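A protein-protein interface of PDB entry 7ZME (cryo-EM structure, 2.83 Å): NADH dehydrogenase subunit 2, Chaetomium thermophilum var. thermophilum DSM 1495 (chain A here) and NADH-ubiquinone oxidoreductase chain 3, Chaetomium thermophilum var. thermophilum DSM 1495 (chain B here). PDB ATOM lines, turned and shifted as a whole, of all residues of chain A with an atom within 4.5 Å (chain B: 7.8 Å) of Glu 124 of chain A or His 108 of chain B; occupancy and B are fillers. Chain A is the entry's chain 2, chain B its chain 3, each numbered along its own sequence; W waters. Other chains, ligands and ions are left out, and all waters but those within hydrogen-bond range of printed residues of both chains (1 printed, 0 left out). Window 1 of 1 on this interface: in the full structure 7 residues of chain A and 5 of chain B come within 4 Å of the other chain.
NE2 of His 108 of chain B lies within hydrogen-bond range of O of Thr 13 of chain A (2.8 Å). The side-chain hydroxyl (OH) of Tyr 104 of chain B lies within hydrogen-bond range of the side-chain carboxylate (OE1) of Glu 124 of chain A (3.0 Å). The backbone carbonyl oxygen of Thr 16 of chain A sits at hydrogen-bond distance from a ring nitrogen (NE2) of His 108 of chain B (3.3 Å).
Among the printed residues, merely in contact across the chains: Ser 14 of chain A with Val 103 of chain B (3.5 Å), Ser 14 of chain A with Tyr 104 of chain B (3.7 Å), Ser 14 of chain A with Gly 107 of chain B (3.2 Å), Ser 14 of chain A with His 108 of chain B (3.8 Å), Leu 17 of chain A with Gly 107 of chain B (3.5 Å), Leu 17 of chain A with His 108 of chain B (3.5 Å) and Glu 124 of chain A with His 108 of chain B (3.1 Å).
Of the printed residues of chain B, Ser 14 of chain A touches Val 103, Tyr 104, Gly 107 and His 108. Ile 123 of chain A touches none of the printed residues of chain B. Of the printed residues of chain A, Gly 107 of chain B touches Ser 14 and Leu 17. His 108 of chain B touches just these residues of chain A: Thr 13, Ser 14, Thr 16, Leu 17 and Glu 124. Lys 112 of chain B touches none of the printed residues of chain A. The nearest printed residue of chain A that does not touch His 108 of chain B is Ile 123 of chain A (4.7 Å).
Hydrophobic or aromatic side chains of chain B that line the printed part of chain A: Val 103, Tyr 104 and His 108. Among the printed residues, 10 pairs touch across the chains.
Water W1 lies within hydrogen-bond range of OH of Tyr 104 of chain B (2.7 Å), OE1 of Glu 124 of chain A (2.9 Å) and ND1 of His 108 of chain B (3.4 Å).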
ATOM      1  N   THR A  13     -10.092  19.359  24.310  1.00  0.00           N
ATOM      2  CA  THR A  13      -9.758  20.628  23.677  1.00  0.00           C
ATOM      3  C   THR A  13      -9.215  21.628  24.688  1.00  0.00           C
ATOM      4  O   THR A  13      -8.359  22.453  24.351  1.00  0.00           O
ATOM      5  CB  THR A  13     -10.993  21.192  22.978  1.00  0.00           C
ATOM      6  OG1 THR A  13     -11.452  20.252  21.999  1.00  0.00           O
ATOM      7  CG2 THR A  13     -10.684  22.514  22.294  1.00  0.00           C
ATOM      8  N   SER A  14      -9.699  21.528  25.929  1.00  0.00           N
ATOM      9  CA  SER A  14      -9.322  22.481  26.998  1.00  0.00           C
ATOM     10  C   SER A  14      -7.862  22.317  27.430  1.00  0.00           C
ATOM     11  O   SER A  14      -7.322  23.263  28.006  1.00  0.00           O
ATOM     12  CB  SER A  14     -10.249  22.314  28.155  1.00  0.00           C
ATOM     13  OG  SER A  14      -9.962  21.125  28.870  1.00  0.00           O
ATOM     14  N   THR A  16      -5.345  21.340  25.320  1.00  0.00           N
ATOM     15  CA  THR A  16      -4.473  21.368  24.121  1.00  0.00           C
ATOM     16  C   THR A  16      -4.469  22.741  23.456  1.00  0.00           C
ATOM     17  O   THR A  16      -5.542  23.346  23.333  1.00  0.00           O
ATOM     18  CB  THR A  16      -4.846  20.286  23.088  1.00  0.00           C
ATOM     19  OG1 THR A  16      -3.828  20.231  22.090  1.00  0.00           O
ATOM     20  CG2 THR A  16      -6.186  20.496  22.422  1.00  0.00           C
ATOM     21  N   LEU A  17      -3.299  23.234  23.084  1.00  0.00           N
ATOM     22  CA  LEU A  17      -3.263  24.473  22.278  1.00  0.00           C
ATOM     23  C   LEU A  17      -2.631  24.057  20.946  1.00  0.00           C
ATOM     24  O   LEU A  17      -2.233  24.947  20.177  1.00  0.00           O
ATOM     25  CB  LEU A  17      -2.475  25.557  23.017  1.00  0.00           C
ATOM     26  CG  LEU A  17      -3.303  26.706  23.582  1.00  0.00           C
ATOM     27  CD1 LEU A  17      -4.280  27.230  22.542  1.00  0.00           C
ATOM     28  CD2 LEU A  17      -4.042  26.268  24.831  1.00  0.00           C
ATOM     29  N   ILE A 122      -8.340  25.230  12.864  1.00  0.00           N
ATOM     30  CA  ILE A 122      -9.252  25.645  13.974  1.00  0.00           C
ATOM     31  C   ILE A 122      -9.545  24.400  14.802  1.00  0.00           C
ATOM     32  O   ILE A 122     -10.045  23.430  14.230  1.00  0.00           O
ATOM     33  CB  ILE A 122     -10.511  26.371  13.458  1.00  0.00           C
ATOM     34  CG1 ILE A 122     -10.143  27.512  12.508  1.00  0.00           C
ATOM     35  CG2 ILE A 122     -11.377  26.849  14.611  1.00  0.00           C
ATOM     36  CD1 ILE A 122     -11.323  28.135  11.819  1.00  0.00           C
ATOM     37  N   ILE A 123      -9.176  24.579  16.189  1.00  0.00           N
ATOM     38  CA  ILE A 123      -9.274  23.407  17.109  1.00  0.00           C
ATOM     39  C   ILE A 123     -10.723  23.204  17.561  1.00  0.00           C
ATOM     40  O   ILE A 123     -11.166  22.049  17.570  1.00  0.00           O
ATOM     41  CB  ILE A 123      -8.311  23.576  18.302  1.00  0.00           C
ATOM     42  CG1 ILE A 123      -6.990  24.227  17.886  1.00  0.00           C
ATOM     43  CG2 ILE A 123      -8.086  22.255  19.015  1.00  0.00           C
ATOM     44  CD1 ILE A 123      -6.053  24.491  19.040  1.00  0.00           C
ATOM     45  N   GLU A 124     -11.479  24.199  17.775  1.00  0.00           N
ATOM     46  CA  GLU A 124     -12.816  24.172  18.420  1.00  0.00           C
ATOM     47  C   GLU A 124     -13.903  24.061  17.359  1.00  0.00           C
ATOM     48  O   GLU A 124     -15.072  24.051  17.737  1.00  0.00           O
ATOM     49  CB  GLU A 124     -13.007  25.427  19.276  1.00  0.00           C
ATOM     50  CG  GLU A 124     -11.939  25.624  20.340  1.00  0.00           C
ATOM     51  CD  GLU A 124     -10.645  26.311  19.924  1.00  0.00           C
ATOM     52  OE1 GLU A 124      -9.872  26.687  20.819  1.00  0.00           O
ATOM     53  OE2 GLU A 124     -10.412  26.478  18.713  1.00  0.00           O
ATOM     54  N   TYR A 125     -13.532  23.971  16.087  1.00  0.00           N
ATOM     55  CA  TYR A 125     -14.536  23.975  14.991  1.00  0.00           C
ATOM     56  C   TYR A 125     -15.508  22.788  15.060  1.00  0.00           C
ATOM     57  O   TYR A 125     -16.708  23.053  14.896  1.00  0.00           O
ATOM     58  CB  TYR A 125     -13.848  24.094  13.629  1.00  0.00           C
ATOM     59  CG  TYR A 125     -14.786  24.174  12.451  1.00  0.00           C
ATOM     60  CD1 TYR A 125     -15.255  25.394  11.998  1.00  0.00           C
ATOM     61  CD2 TYR A 125     -15.209  23.032  11.788  1.00  0.00           C
ATOM     62  CE1 TYR A 125     -16.119  25.482  10.921  1.00  0.00           C
ATOM     63  CE2 TYR A 125     -16.080  23.101  10.714  1.00  0.00           C
ATOM     64  CZ  TYR A 125     -16.533  24.331  10.278  1.00  0.00           C
ATOM     65  OH  TYR A 125     -17.382  24.421   9.216  1.00  0.00           O
ATOM     66  N   PRO A 126     -15.106  21.522  15.322  1.00  0.00           N
ATOM     67  CA  PRO A 126     -16.079  20.436  15.345  1.00  0.00           C
ATOM     68  C   PRO A 126     -16.852  20.529  16.666  1.00  0.00           C
ATOM     69  O   PRO A 126     -17.954  20.055  16.729  1.00  0.00           O
ATOM     70  CB  PRO A 126     -15.204  19.174  15.365  1.00  0.00           C
ATOM     71  CG  PRO A 126     -13.916  19.621  16.003  1.00  0.00           C
ATOM     72  CD  PRO A 126     -13.731  21.032  15.496  1.00  0.00           C
ATOM     73  N   LEU A 127     -16.267  21.193  17.656  1.00  0.00           N
ATOM     74  CA  LEU A 127     -16.909  21.343  18.953  1.00  0.00           C
ATOM     75  C   LEU A 127     -18.081  22.313  18.879  1.00  0.00           C
ATOM     76  O   LEU A 127     -19.166  22.033  19.398  1.00  0.00           O
ATOM     77  CB  LEU A 127     -15.866  21.809  19.964  1.00  0.00           C
ATOM     78  CG  LEU A 127     -16.157  21.779  21.456  1.00  0.00           C
ATOM     79  CD1 LEU A 127     -14.873  21.415  22.140  1.00  0.00           C
ATOM     80  CD2 LEU A 127     -16.648  23.128  21.928  1.00  0.00           C
ATOM     81  N   ILE A 128     -17.905  23.427  18.159  1.00  0.00           N
ATOM     82  CA  ILE A 128     -18.967  24.469  17.995  1.00  0.00           C
ATOM     83  C   ILE A 128     -20.076  23.913  17.094  1.00  0.00           C
ATOM     84  O   ILE A 128     -21.239  24.258  17.317  1.00  0.00           O
ATOM     85  CB  ILE A 128     -18.378  25.805  17.502  1.00  0.00           C
ATOM     86  CG1 ILE A 128     -17.360  26.357  18.504  1.00  0.00           C
ATOM     87  CG2 ILE A 128     -19.470  26.823  17.214  1.00  0.00           C
ATOM     88  CD1 ILE A 128     -17.160  27.849  18.421  1.00  0.00           C
ATOM     89  N   PHE B 102     -14.880  26.689  32.585  1.00  0.00           N
ATOM     90  CA  PHE B 102     -13.793  27.357  33.342  1.00  0.00           C
ATOM     91  C   PHE B 102     -12.458  26.659  33.073  1.00  0.00           C
ATOM     92  O   PHE B 102     -11.444  27.344  32.956  1.00  0.00           O
ATOM     93  CB  PHE B 102     -14.145  27.365  34.834  1.00  0.00           C
ATOM     94  CG  PHE B 102     -13.295  28.258  35.698  1.00  0.00           C
ATOM     95  CD1 PHE B 102     -13.029  29.564  35.325  1.00  0.00           C
ATOM     96  CD2 PHE B 102     -12.784  27.798  36.898  1.00  0.00           C
ATOM     97  CE1 PHE B 102     -12.252  30.384  36.128  1.00  0.00           C
ATOM     98  CE2 PHE B 102     -12.014  28.620  37.702  1.00  0.00           C
ATOM     99  CZ  PHE B 102     -11.750  29.911  37.315  1.00  0.00           C
ATOM    100  N   VAL B 103     -12.469  25.336  32.972  1.00  0.00           N
ATOM    101  CA  VAL B 103     -11.225  24.552  32.729  1.00  0.00           C
ATOM    102  C   VAL B 103     -10.746  24.962  31.335  1.00  0.00           C
ATOM    103  O   VAL B 103      -9.523  25.050  31.130  1.00  0.00           O
ATOM    104  CB  VAL B 103     -11.507  23.037  32.826  1.00  0.00           C
ATOM    105  CG1 VAL B 103     -10.402  22.188  32.213  1.00  0.00           C
ATOM    106  CG2 VAL B 103     -11.805  22.596  34.246  1.00  0.00           C
ATOM    107  N   TYR B 104     -11.679  25.208  30.412  1.00  0.00           N
ATOM    108  CA  TYR B 104     -11.306  25.701  29.061  1.00  0.00           C
ATOM    109  C   TYR B 104     -10.616  27.063  29.163  1.00  0.00           C
ATOM    110  O   TYR B 104      -9.636  27.285  28.443  1.00  0.00           O
ATOM    111  CB  TYR B 104     -12.548  25.779  28.174  1.00  0.00           C
ATOM    112  CG  TYR B 104     -12.297  26.332  26.794  1.00  0.00           C
ATOM    113  CD1 TYR B 104     -12.468  27.680  26.525  1.00  0.00           C
ATOM    114  CD2 TYR B 104     -11.878  25.512  25.760  1.00  0.00           C
ATOM    115  CE1 TYR B 104     -12.225  28.199  25.266  1.00  0.00           C
ATOM    116  CE2 TYR B 104     -11.640  26.014  24.493  1.00  0.00           C
ATOM    117  CZ  TYR B 104     -11.811  27.364  24.247  1.00  0.00           C
ATOM    118  OH  TYR B 104     -11.580  27.878  23.007  1.00  0.00           O
ATOM    119  N   GLU B 105     -11.121  27.951  30.021  1.00  0.00           N
ATOM    120  CA  GLU B 105     -10.514  29.295  30.210  1.00  0.00           C
ATOM    121  C   GLU B 105      -9.101  29.184  30.796  1.00  0.00           C
ATOM    122  O   GLU B 105      -8.247  29.994  30.420  1.00  0.00           O
ATOM    123  CB  GLU B 105     -11.397  30.208  31.066  1.00  0.00           C
ATOM    124  CG  GLU B 105     -12.880  30.121  30.772  1.00  0.00           C
ATOM    125  CD  GLU B 105     -13.312  30.398  29.345  1.00  0.00           C
ATOM    126  OE1 GLU B 105     -14.424  29.985  28.985  1.00  0.00           O
ATOM    127  OE2 GLU B 105     -12.542  31.026  28.604  1.00  0.00           O
ATOM    128  N   LEU B 106      -8.913  28.259  31.731  1.00  0.00           N
ATOM    129  CA  LEU B 106      -7.599  28.087  32.379  1.00  0.00           C
ATOM    130  C   LEU B 106      -6.637  27.409  31.403  1.00  0.00           C
ATOM    131  O   LEU B 106      -5.516  27.901  31.261  1.00  0.00           O
ATOM    132  CB  LEU B 106      -7.779  27.284  33.669  1.00  0.00           C
ATOM    133  CG  LEU B 106      -8.656  27.929  34.741  1.00  0.00           C
ATOM    134  CD1 LEU B 106      -9.099  26.901  35.768  1.00  0.00           C
ATOM    135  CD2 LEU B 106      -7.935  29.081  35.417  1.00  0.00           C
ATOM    136  N   GLY B 107      -7.040  26.303  30.787  1.00  0.00           N
ATOM    137  CA  GLY B 107      -6.139  25.565  29.888  1.00  0.00           C
ATOM    138  C   GLY B 107      -5.714  26.381  28.686  1.00  0.00           C
ATOM    139  O   GLY B 107      -4.556  26.256  28.281  1.00  0.00           O
ATOM    140  N   HIS B 108      -6.625  27.157  28.108  1.00  0.00           N
ATOM    141  CA  HIS B 108      -6.307  27.951  26.893  1.00  0.00           C
ATOM    142  C   HIS B 108      -5.547  29.214  27.300  1.00  0.00           C
ATOM    143  O   HIS B 108      -5.123  29.949  26.389  1.00  0.00           O
ATOM    144  CB  HIS B 108      -7.554  28.165  26.030  1.00  0.00           C
ATOM    145  CG  HIS B 108      -7.781  27.059  25.059  1.00  0.00           C
ATOM    146  ND1 HIS B 108      -7.576  27.218  23.707  1.00  0.00           N
ATOM    147  CD2 HIS B 108      -8.160  25.778  25.239  1.00  0.00           C
ATOM    148  CE1 HIS B 108      -7.833  26.086  23.091  1.00  0.00           C
ATOM    149  NE2 HIS B 108      -8.197  25.191  24.009  1.00  0.00           N
ATOM    150  N   ASP B 109      -5.399  29.453  28.605  1.00  0.00           N
ATOM    151  CA  ASP B 109      -4.588  30.584  29.130  1.00  0.00           C
ATOM    152  C   ASP B 109      -5.239  31.910  28.748  1.00  0.00           C
ATOM    153  O   ASP B 109      -4.504  32.886  28.529  1.00  0.00           O
ATOM    154  CB  ASP B 109      -3.109  30.491  28.737  1.00  0.00           C
ATOM    155  CG  ASP B 109      -2.349  29.374  29.429  1.00  0.00           C
ATOM    156  OD1 ASP B 109      -2.905  28.782  30.370  1.00  0.00           O
ATOM    157  OD2 ASP B 109      -1.201  29.109  29.021  1.00  0.00           O
ATOM    158  N   ALA B 110      -6.563  31.930  28.650  1.00  0.00           N
ATOM    159  CA  ALA B 110      -7.294  33.172  28.315  1.00  0.00           C
ATOM    160  C   ALA B 110      -7.041  34.220  29.397  1.00  0.00           C
ATOM    161  O   ALA B 110      -6.951  35.402  29.056  1.00  0.00           O
ATOM    162  CB  ALA B 110      -8.763  32.857  28.201  1.00  0.00           C
ATOM    163  N   LEU B 111      -6.987  33.793  30.657  1.00  0.00           N
ATOM    164  CA  LEU B 111      -6.779  34.716  31.795  1.00  0.00           C
ATOM    165  C   LEU B 111      -5.295  34.773  32.180  1.00  0.00           C
ATOM    166  O   LEU B 111      -5.014  34.522  33.365  1.00  0.00           O
ATOM    167  CB  LEU B 111      -7.628  34.169  32.942  1.00  0.00           C
ATOM    168  CG  LEU B 111      -9.032  33.696  32.564  1.00  0.00           C
ATOM    169  CD1 LEU B 111      -9.555  32.678  33.564  1.00  0.00           C
ATOM    170  CD2 LEU B 111      -9.990  34.869  32.436  1.00  0.00           C
ATOM    171  N   LYS B 112      -4.382  35.115  31.265  1.00  0.00           N
ATOM    172  CA  LYS B 112      -2.954  35.069  31.571  1.00  0.00           C
ATOM    173  C   LYS B 112      -2.208  36.157  30.793  1.00  0.00           C
ATOM    174  O   LYS B 112      -1.237  35.885  30.088  1.00  0.00           O
ATOM    175  CB  LYS B 112      -2.370  33.691  31.267  1.00  0.00           C
ATOM    176  CG  LYS B 112      -1.093  33.376  32.035  1.00  0.00           C
ATOM    177  CD  LYS B 112      -0.257  32.330  31.316  1.00  0.00           C
ATOM    178  CE  LYS B 112       0.181  32.822  29.945  1.00  0.00           C
ATOM    179  NZ  LYS B 112       1.056  34.023  30.038  1.00  0.00           N
HETATM  180  O   HOH W   1      -9.553  29.328  21.864  1.00  0.00           O
